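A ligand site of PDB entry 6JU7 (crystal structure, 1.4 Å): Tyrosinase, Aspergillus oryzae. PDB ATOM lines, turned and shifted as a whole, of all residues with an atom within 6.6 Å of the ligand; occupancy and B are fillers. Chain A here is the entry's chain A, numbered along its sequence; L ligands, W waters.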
ATOM      1  N   HIS A  71       0.238 -15.310  18.692  1.00  0.00           N
ATOM      2  CA  HIS A  71      -0.237 -14.546  17.533  1.00  0.00           C
ATOM      3  C   HIS A  71      -0.916 -15.422  16.491  1.00  0.00           C
ATOM      4  O   HIS A  71      -1.989 -15.095  15.967  1.00  0.00           O
ATOM      5  CB  HIS A  71       0.982 -13.817  16.935  1.00  0.00           C
ATOM      6  CG  HIS A  71       0.632 -12.815  15.897  1.00  0.00           C
ATOM      7  ND1 HIS A  71       0.840 -13.056  14.553  1.00  0.00           N
ATOM      8  CD2 HIS A  71       0.135 -11.551  15.977  1.00  0.00           C
ATOM      9  CE1 HIS A  71       0.459 -12.010  13.851  1.00  0.00           C
ATOM     10  NE2 HIS A  71       0.028 -11.073  14.677  1.00  0.00           N
ATOM     11  N   HIS A  98      -6.926  -9.464  13.467  1.00  0.00           N
ATOM     12  CA  HIS A  98      -6.697  -8.753  12.222  1.00  0.00           C
ATOM     13  C   HIS A  98      -8.026  -8.498  11.526  1.00  0.00           C
ATOM     14  O   HIS A  98      -8.960  -9.285  11.690  1.00  0.00           O
ATOM     15  CB  HIS A  98      -5.749  -9.519  11.284  1.00  0.00           C
ATOM     16  CG  HIS A  98      -4.398  -9.666  11.916  1.00  0.00           C
ATOM     17  ND1 HIS A  98      -3.961 -10.784  12.596  1.00  0.00           N
ATOM     18  CD2 HIS A  98      -3.365  -8.767  11.962  1.00  0.00           C
ATOM     19  CE1 HIS A  98      -2.727 -10.572  13.040  1.00  0.00           C
ATOM     20  NE2 HIS A  98      -2.345  -9.354  12.659  1.00  0.00           N
ATOM     21  N   PHE A 103      -7.984  -4.427  16.286  1.00  0.00           N
ATOM     22  CA  PHE A 103      -6.589  -4.688  15.886  1.00  0.00           C
ATOM     23  C   PHE A 103      -5.625  -3.867  16.721  1.00  0.00           C
ATOM     24  O   PHE A 103      -4.635  -4.412  17.237  1.00  0.00           O
ATOM     25  CB  PHE A 103      -6.463  -4.389  14.373  1.00  0.00           C
ATOM     26  CG  PHE A 103      -5.033  -4.199  13.922  1.00  0.00           C
ATOM     27  CD1 PHE A 103      -4.150  -5.252  13.746  1.00  0.00           C
ATOM     28  CD2 PHE A 103      -4.569  -2.915  13.650  1.00  0.00           C
ATOM     29  CE1 PHE A 103      -2.833  -5.035  13.375  1.00  0.00           C
ATOM     30  CE2 PHE A 103      -3.252  -2.687  13.315  1.00  0.00           C
ATOM     31  CZ  PHE A 103      -2.378  -3.758  13.181  1.00  0.00           C
ATOM     32  N   HIS A 107      -3.183  -5.699  19.873  1.00  0.00           N
ATOM     33  CA  HIS A 107      -1.724  -5.635  19.747  1.00  0.00           C
ATOM     34  C   HIS A 107      -1.102  -4.737  20.809  1.00  0.00           C
ATOM     35  O   HIS A 107       0.030  -5.019  21.208  1.00  0.00           O
ATOM     36  CB  HIS A 107      -1.335  -5.180  18.326  1.00  0.00           C
ATOM     37  CG  HIS A 107      -1.542  -6.303  17.331  1.00  0.00           C
ATOM     38  ND1 HIS A 107      -2.728  -6.571  16.682  1.00  0.00           N
ATOM     39  CD2 HIS A 107      -0.667  -7.266  16.940  1.00  0.00           C
ATOM     40  CE1 HIS A 107      -2.574  -7.627  15.903  1.00  0.00           C
ATOM     41  NE2 HIS A 107      -1.328  -8.076  16.040  1.00  0.00           N
ATOM     42  N   THR A 220      -0.586 -19.376   0.831  1.00  0.00           N
ATOM     43  CA  THR A 220      -0.743 -17.967   0.495  1.00  0.00           C
ATOM     44  C   THR A 220      -1.103 -17.817  -0.975  1.00  0.00           C
ATOM     45  O   THR A 220      -0.853 -18.695  -1.780  1.00  0.00           O
ATOM     46  CB  THR A 220       0.595 -17.229   0.771  1.00  0.00           C
ATOM     47  OG1 THR A 220       0.394 -15.814   0.758  1.00  0.00           O
ATOM     48  CG2 THR A 220       1.601 -17.546  -0.320  1.00  0.00           C
ATOM     49  N   TYR A 271       0.253  -2.826  -1.870  1.00  0.00           N
ATOM     50  CA  TYR A 271      -0.543  -3.859  -2.557  1.00  0.00           C
ATOM     51  C   TYR A 271      -1.893  -3.305  -2.988  1.00  0.00           C
ATOM     52  O   TYR A 271      -2.542  -3.857  -3.878  1.00  0.00           O
ATOM     53  CB  TYR A 271      -0.687  -5.133  -1.733  1.00  0.00           C
ATOM     54  CG  TYR A 271      -1.519  -5.032  -0.472  1.00  0.00           C
ATOM     55  CD1 TYR A 271      -2.899  -5.143  -0.473  1.00  0.00           C
ATOM     56  CD2 TYR A 271      -0.887  -4.849   0.756  1.00  0.00           C
ATOM     57  CE1 TYR A 271      -3.629  -5.054   0.710  1.00  0.00           C
ATOM     58  CE2 TYR A 271      -1.601  -4.762   1.920  1.00  0.00           C
ATOM     59  CZ  TYR A 271      -2.976  -4.860   1.901  1.00  0.00           C
ATOM     60  OH  TYR A 271      -3.662  -4.761   3.092  1.00  0.00           O
ATOM     61  N   GLU A 329      -4.006  -0.224   9.868  1.00  0.00           N
ATOM     62  CA  GLU A 329      -3.786  -1.657   9.650  1.00  0.00           C
ATOM     63  C   GLU A 329      -3.275  -1.894   8.236  1.00  0.00           C
ATOM     64  O   GLU A 329      -2.382  -2.723   8.030  1.00  0.00           O
ATOM     65  CB  GLU A 329      -5.091  -2.421   9.900  1.00  0.00           C
ATOM     66  CG  GLU A 329      -4.897  -3.924   9.882  1.00  0.00           C
ATOM     67  CD  GLU A 329      -6.145  -4.732  10.224  1.00  0.00           C
ATOM     68  OE1 GLU A 329      -7.267  -4.178  10.351  1.00  0.00           O
ATOM     69  OE2 GLU A 329      -5.952  -5.970  10.359  1.00  0.00           O
ATOM     70  N   HIS A 332       0.355  -1.045   8.134  1.00  0.00           N
ATOM     71  CA  HIS A 332       1.058  -2.121   8.839  1.00  0.00           C
ATOM     72  C   HIS A 332       1.161  -3.373   7.981  1.00  0.00           C
ATOM     73  O   HIS A 332       2.189  -4.060   8.037  1.00  0.00           O
ATOM     74  CB  HIS A 332       0.340  -2.372  10.163  1.00  0.00           C
ATOM     75  CG  HIS A 332       0.129  -3.777  10.594  1.00  0.00           C
ATOM     76  ND1 HIS A 332      -0.881  -4.582  10.116  1.00  0.00           N
ATOM     77  CD2 HIS A 332       0.771  -4.523  11.533  1.00  0.00           C
ATOM     78  CE1 HIS A 332      -0.840  -5.760  10.714  1.00  0.00           C
ATOM     79  NE2 HIS A 332       0.159  -5.767  11.575  1.00  0.00           N
ATOM     80  N   ASN A 333       0.121  -3.705   7.224  1.00  0.00           N
ATOM     81  CA  ASN A 333       0.148  -4.883   6.356  1.00  0.00           C
ATOM     82  C   ASN A 333       1.256  -4.771   5.309  1.00  0.00           C
ATOM     83  O   ASN A 333       2.031  -5.713   5.083  1.00  0.00           O
ATOM     84  CB  ASN A 333      -1.189  -5.003   5.619  1.00  0.00           C
ATOM     85  CG  ASN A 333      -2.334  -5.506   6.487  1.00  0.00           C
ATOM     86  OD1 ASN A 333      -2.155  -5.898   7.638  1.00  0.00           O
ATOM     87  ND2 ASN A 333      -3.528  -5.472   5.928  1.00  0.00           N
ATOM     88  N   ASN A 334       1.358  -3.614   4.666  1.00  0.00           N
ATOM     89  CA  ASN A 334       2.437  -3.380   3.702  1.00  0.00           C
ATOM     90  C   ASN A 334       3.810  -3.448   4.340  1.00  0.00           C
ATOM     91  O   ASN A 334       4.748  -4.068   3.815  1.00  0.00           O
ATOM     92  CB  ASN A 334       2.215  -2.001   3.056  1.00  0.00           C
ATOM     93  CG  ASN A 334       1.148  -2.063   1.985  1.00  0.00           C
ATOM     94  OD1 ASN A 334       1.402  -2.518   0.876  1.00  0.00           O
ATOM     95  ND2 ASN A 334      -0.039  -1.580   2.323  1.00  0.00           N
ATOM     96  N   HIS A 336       4.760  -5.149   6.952  1.00  0.00           N
ATOM     97  CA  HIS A 336       5.056  -6.564   7.190  1.00  0.00           C
ATOM     98  C   HIS A 336       5.558  -7.227   5.920  1.00  0.00           C
ATOM     99  O   HIS A 336       6.551  -7.942   5.923  1.00  0.00           O
ATOM    100  CB  HIS A 336       3.792  -7.301   7.662  1.00  0.00           C
ATOM    101  CG  HIS A 336       3.605  -7.349   9.146  1.00  0.00           C
ATOM    102  ND1 HIS A 336       4.229  -8.323   9.905  1.00  0.00           N
ATOM    103  CD2 HIS A 336       2.874  -6.619  10.007  1.00  0.00           C
ATOM    104  CE1 HIS A 336       3.899  -8.158  11.181  1.00  0.00           C
ATOM    105  NE2 HIS A 336       3.077  -7.132  11.277  1.00  0.00           N
ATOM    106  N   ASN A 337       4.841  -7.023   4.808  1.00  0.00           N
ATOM    107  CA  ASN A 337       5.260  -7.596   3.542  1.00  0.00           C
ATOM    108  C   ASN A 337       6.657  -7.157   3.093  1.00  0.00           C
ATOM    109  O   ASN A 337       7.461  -7.978   2.600  1.00  0.00           O
ATOM    110  CB  ASN A 337       4.232  -7.207   2.473  1.00  0.00           C
ATOM    111  CG  ASN A 337       2.913  -7.963   2.600  1.00  0.00           C
ATOM    112  OD1 ASN A 337       2.836  -8.989   3.264  1.00  0.00           O
ATOM    113  ND2 ASN A 337       1.879  -7.405   1.962  1.00  0.00           N
ATOM    114  N   PHE A 342       7.518 -10.877   0.270  1.00  0.00           N
ATOM    115  CA  PHE A 342       6.143 -11.266  -0.053  1.00  0.00           C
ATOM    116  C   PHE A 342       5.992 -12.023  -1.360  1.00  0.00           C
ATOM    117  O   PHE A 342       4.865 -12.300  -1.796  1.00  0.00           O
ATOM    118  CB  PHE A 342       5.278  -9.984  -0.065  1.00  0.00           C
ATOM    119  CG  PHE A 342       5.797  -8.929  -1.004  1.00  0.00           C
ATOM    120  CD1 PHE A 342       5.272  -8.800  -2.285  1.00  0.00           C
ATOM    121  CD2 PHE A 342       6.810  -8.050  -0.625  1.00  0.00           C
ATOM    122  CE1 PHE A 342       5.743  -7.863  -3.174  1.00  0.00           C
ATOM    123  CE2 PHE A 342       7.291  -7.112  -1.516  1.00  0.00           C
ATOM    124  CZ  PHE A 342       6.766  -6.998  -2.796  1.00  0.00           C
ATOM    125  N   HIS A 359       9.262 -14.679   7.079  1.00  0.00           N
ATOM    126  CA  HIS A 359       8.267 -14.822   8.120  1.00  0.00           C
ATOM    127  C   HIS A 359       7.379 -13.595   8.320  1.00  0.00           C
ATOM    128  O   HIS A 359       6.170 -13.734   8.526  1.00  0.00           O
ATOM    129  CB  HIS A 359       8.962 -15.174   9.447  1.00  0.00           C
ATOM    130  CG  HIS A 359       9.535 -16.562   9.377  1.00  0.00           C
ATOM    131  ND1 HIS A 359      10.603 -16.901   8.581  1.00  0.00           N
ATOM    132  CD2 HIS A 359       9.162 -17.701  10.019  1.00  0.00           C
ATOM    133  CE1 HIS A 359      10.850 -18.207   8.724  1.00  0.00           C
ATOM    134  NE2 HIS A 359      10.000 -18.705   9.605  1.00  0.00           N
ATOM    135  N   MET A 360       7.962 -12.399   8.248  1.00  0.00           N
ATOM    136  CA  MET A 360       7.171 -11.211   8.574  1.00  0.00           C
ATOM    137  C   MET A 360       6.033 -10.967   7.590  1.00  0.00           C
ATOM    138  O   MET A 360       5.113 -10.204   7.923  1.00  0.00           O
ATOM    139  CB  MET A 360       8.064  -9.961   8.683  1.00  0.00           C
ATOM    140  CG  MET A 360       8.693  -9.756  10.050  1.00  0.00           C
ATOM    141  SD  MET A 360       7.525  -9.124  11.273  1.00  0.00           S
ATOM    142  CE  MET A 360       7.433  -7.396  10.770  1.00  0.00           C
ATOM    143  N   SER A 361       6.028 -11.576   6.402  1.00  0.00           N
ATOM    144  CA  SER A 361       4.905 -11.339   5.474  1.00  0.00           C
ATOM    145  C   SER A 361       3.725 -12.255   5.722  1.00  0.00           C
ATOM    146  O   SER A 361       2.708 -12.123   5.021  1.00  0.00           O
ATOM    147  CB  SER A 361       5.331 -11.506   4.023  1.00  0.00           C
ATOM    148  OG  SER A 361       5.532 -12.882   3.736  1.00  0.00           O
ATOM    149  N   SER A 362       3.847 -13.160   6.693  1.00  0.00           N
ATOM    150  CA  SER A 362       2.846 -14.211   6.871  1.00  0.00           C
ATOM    151  C   SER A 362       2.263 -14.170   8.277  1.00  0.00           C
ATOM    152  O   SER A 362       2.960 -14.448   9.241  1.00  0.00           O
ATOM    153  CB  SER A 362       3.527 -15.554   6.594  1.00  0.00           C
ATOM    154  OG  SER A 362       2.655 -16.645   6.823  1.00  0.00           O
ATOM    155  N   VAL A 363       0.976 -13.822   8.401  1.00  0.00           N
ATOM    156  CA  VAL A 363       0.336 -13.728   9.720  1.00  0.00           C
ATOM    157  C   VAL A 363       0.653 -14.921  10.598  1.00  0.00           C
ATOM    158  O   VAL A 363       0.993 -14.747  11.783  1.00  0.00           O
ATOM    159  CB  VAL A 363      -1.191 -13.569   9.572  1.00  0.00           C
ATOM    160  CG1 VAL A 363      -1.923 -13.808  10.884  1.00  0.00           C
ATOM    161  CG2 VAL A 363      -1.499 -12.175   9.029  1.00  0.00           C
ATOM    162  N   PRO A 364       0.537 -16.172  10.148  1.00  0.00           N
ATOM    163  CA  PRO A 364       0.778 -17.293  11.053  1.00  0.00           C
ATOM    164  C   PRO A 364       2.156 -17.348  11.674  1.00  0.00           C
ATOM    165  O   PRO A 364       2.252 -17.966  12.743  1.00  0.00           O
ATOM    166  CB  PRO A 364       0.516 -18.518  10.190  1.00  0.00           C
ATOM    167  CG  PRO A 364      -0.331 -18.049   9.067  1.00  0.00           C
ATOM    168  CD  PRO A 364       0.019 -16.609   8.838  1.00  0.00           C
ATOM    169  N   ALA A 366       4.681 -14.488  11.538  1.00  0.00           N
ATOM    170  CA  ALA A 366       5.416 -13.235  11.601  1.00  0.00           C
ATOM    171  C   ALA A 366       5.987 -12.966  12.984  1.00  0.00           C
ATOM    172  O   ALA A 366       7.056 -12.341  13.112  1.00  0.00           O
ATOM    173  CB  ALA A 366       4.507 -12.094  11.168  1.00  0.00           C
ATOM    174  N   ALA A 367       5.314 -13.378  14.057  1.00  0.00           N
ATOM    175  CA  ALA A 367       5.721 -13.005  15.413  1.00  0.00           C
ATOM    176  C   ALA A 367       7.007 -13.702  15.798  1.00  0.00           C
ATOM    177  O   ALA A 367       7.674 -13.250  16.747  1.00  0.00           O
ATOM    178  CB  ALA A 367       4.576 -13.267  16.399  1.00  0.00           C
ATOM    179  N   PHE A 372       9.221  -8.165  14.623  1.00  0.00           N
ATOM    180  CA  PHE A 372       7.757  -8.067  14.737  1.00  0.00           C
ATOM    181  C   PHE A 372       7.375  -7.117  15.851  1.00  0.00           C
ATOM    182  O   PHE A 372       6.509  -6.248  15.712  1.00  0.00           O
ATOM    183  CB  PHE A 372       7.224  -9.462  15.056  1.00  0.00           C
ATOM    184  CG  PHE A 372       5.747  -9.497  15.383  1.00  0.00           C
ATOM    185  CD1 PHE A 372       5.306  -9.306  16.672  1.00  0.00           C
ATOM    186  CD2 PHE A 372       4.824  -9.738  14.376  1.00  0.00           C
ATOM    187  CE1 PHE A 372       3.957  -9.297  16.973  1.00  0.00           C
ATOM    188  CE2 PHE A 372       3.471  -9.730  14.663  1.00  0.00           C
ATOM    189  CZ  PHE A 372       3.035  -9.552  15.967  1.00  0.00           C
ATOM    190  N   HIS A 376       5.479  -3.592  15.815  1.00  0.00           N
ATOM    191  CA  HIS A 376       4.222  -3.391  16.524  1.00  0.00           C
ATOM    192  C   HIS A 376       4.338  -2.365  17.638  1.00  0.00           C
ATOM    193  O   HIS A 376       3.362  -1.695  17.990  1.00  0.00           O
ATOM    194  CB  HIS A 376       3.717  -4.740  17.059  1.00  0.00           C
ATOM    195  CG  HIS A 376       2.881  -5.377  15.980  1.00  0.00           C
ATOM    196  ND1 HIS A 376       1.564  -5.038  15.773  1.00  0.00           N
ATOM    197  CD2 HIS A 376       3.222  -6.215  14.982  1.00  0.00           C
ATOM    198  CE1 HIS A 376       1.097  -5.715  14.714  1.00  0.00           C
ATOM    199  NE2 HIS A 376       2.100  -6.457  14.230  1.00  0.00           N
HETATM  200  N1  LIG L   1       0.582 -10.471   4.295  1.00  0.00           N
HETATM  201  C1  LIG L   1      -0.472  -9.613   4.823  1.00  0.00           C
HETATM  202  C2  LIG L   1      -1.160  -8.856   3.680  1.00  0.00           C
HETATM  203  O1  LIG L   1      -2.236  -8.257   3.936  1.00  0.00           O
HETATM  204  C3  LIG L   1       0.084  -8.586   5.799  1.00  0.00           C
HETATM  205  C4  LIG L   1       0.425  -9.043   7.194  1.00  0.00           C
HETATM  206  C5  LIG L   1       1.472  -9.931   7.425  1.00  0.00           C
HETATM  207  C6  LIG L   1      -0.282  -8.558   8.284  1.00  0.00           C
HETATM  208  C7  LIG L   1       1.773 -10.338   8.714  1.00  0.00           C
HETATM  209  C8  LIG L   1       0.020  -8.943   9.578  1.00  0.00           C
HETATM  210  C9  LIG L   1       1.051  -9.834   9.784  1.00  0.00           C
HETATM  211  O2  LIG L   1       1.374 -10.236  11.044  1.00  0.00           O
HETATM  212  O3  LIG L   1      -0.601  -8.881   2.559  1.00  0.00           O
HETATM  213  O   HOH W   1      -4.001  -9.772   5.529  1.00  0.00           O
HETATM  214  O   HOH W   2      -0.443 -13.003   6.020  1.00  0.00           O
HETATM  215  O   HOH W   3      -0.925 -12.193   2.345  1.00  0.00           O
HETATM  216  O   HOH W   4       0.341  -8.554  12.892  1.00  0.00           O
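N of Ala 366 sits close to O of His 359 (3.4 Å).
The side-chain amide oxygen (OD1) of Asn 333 sits at hydrogen-bond distance from a ring nitrogen (ND1) of His 332 (3.1 Å).
O of Glu 329 sits at hydrogen-bond distance from ND1 of His 332, at 3.2 Å.
The side-chain amide oxygen (OD1) of Asn 333 sits close to the backbone carbonyl oxygen (O) of Glu 329.
NE2 of His 332 lies close to NE2 of His 376 (3.4 Å).
O of Val 363 lies within hydrogen-bond range of ND1 of His 71 (3.2 Å).
A ring nitrogen (NE2) of His 376 lies within hydrogen-bond range of a ring nitrogen (NE2) of His 336, at 3.2 Å.
ND2 of Asn 333 sits at hydrogen-bond distance from OH of Tyr 271.
A nitrogen (N1) of the ligand lies within hydrogen-bond range of the side-chain amide oxygen (OD1) of Asn 337 (2.9 Å).
A nitrogen (N1) of the ligand is in hydrogen-bond range of the backbone carbonyl oxygen (O) of Ser 361 (2.8 Å).
Merely in contact with the ligand: His 336, Asn 333, Met 360, His 71, His 332, Val 363, Ala 366, Tyr 271, Ser 362 and His 98.
Hydrophobic or aromatic side chains within 4 Å of the ligand: His 71, His 332, His 336, Val 363 and Ala 366.
Of the 23 residues printed, 12 come within 4 Å of the ligand.
The nearest printed residue that does not touch the ligand is Phe 372 (4.2 Å).
Water W4 lies within hydrogen-bond range of O2 of the ligand (2.7 Å), NE2 of His 98 (2.8 Å), NE2 of His 376 (3.0 Å), NE2 of His 332 (3.1 Å), NE2 of His 71 (3.1 Å) and NE2 of His 336 (3.5 Å).
Water W2 lies within hydrogen-bond range of N of Val 363 (2.9 Å), N1 of the ligand (3.2 Å) and O of Ser 361 (3.4 Å).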
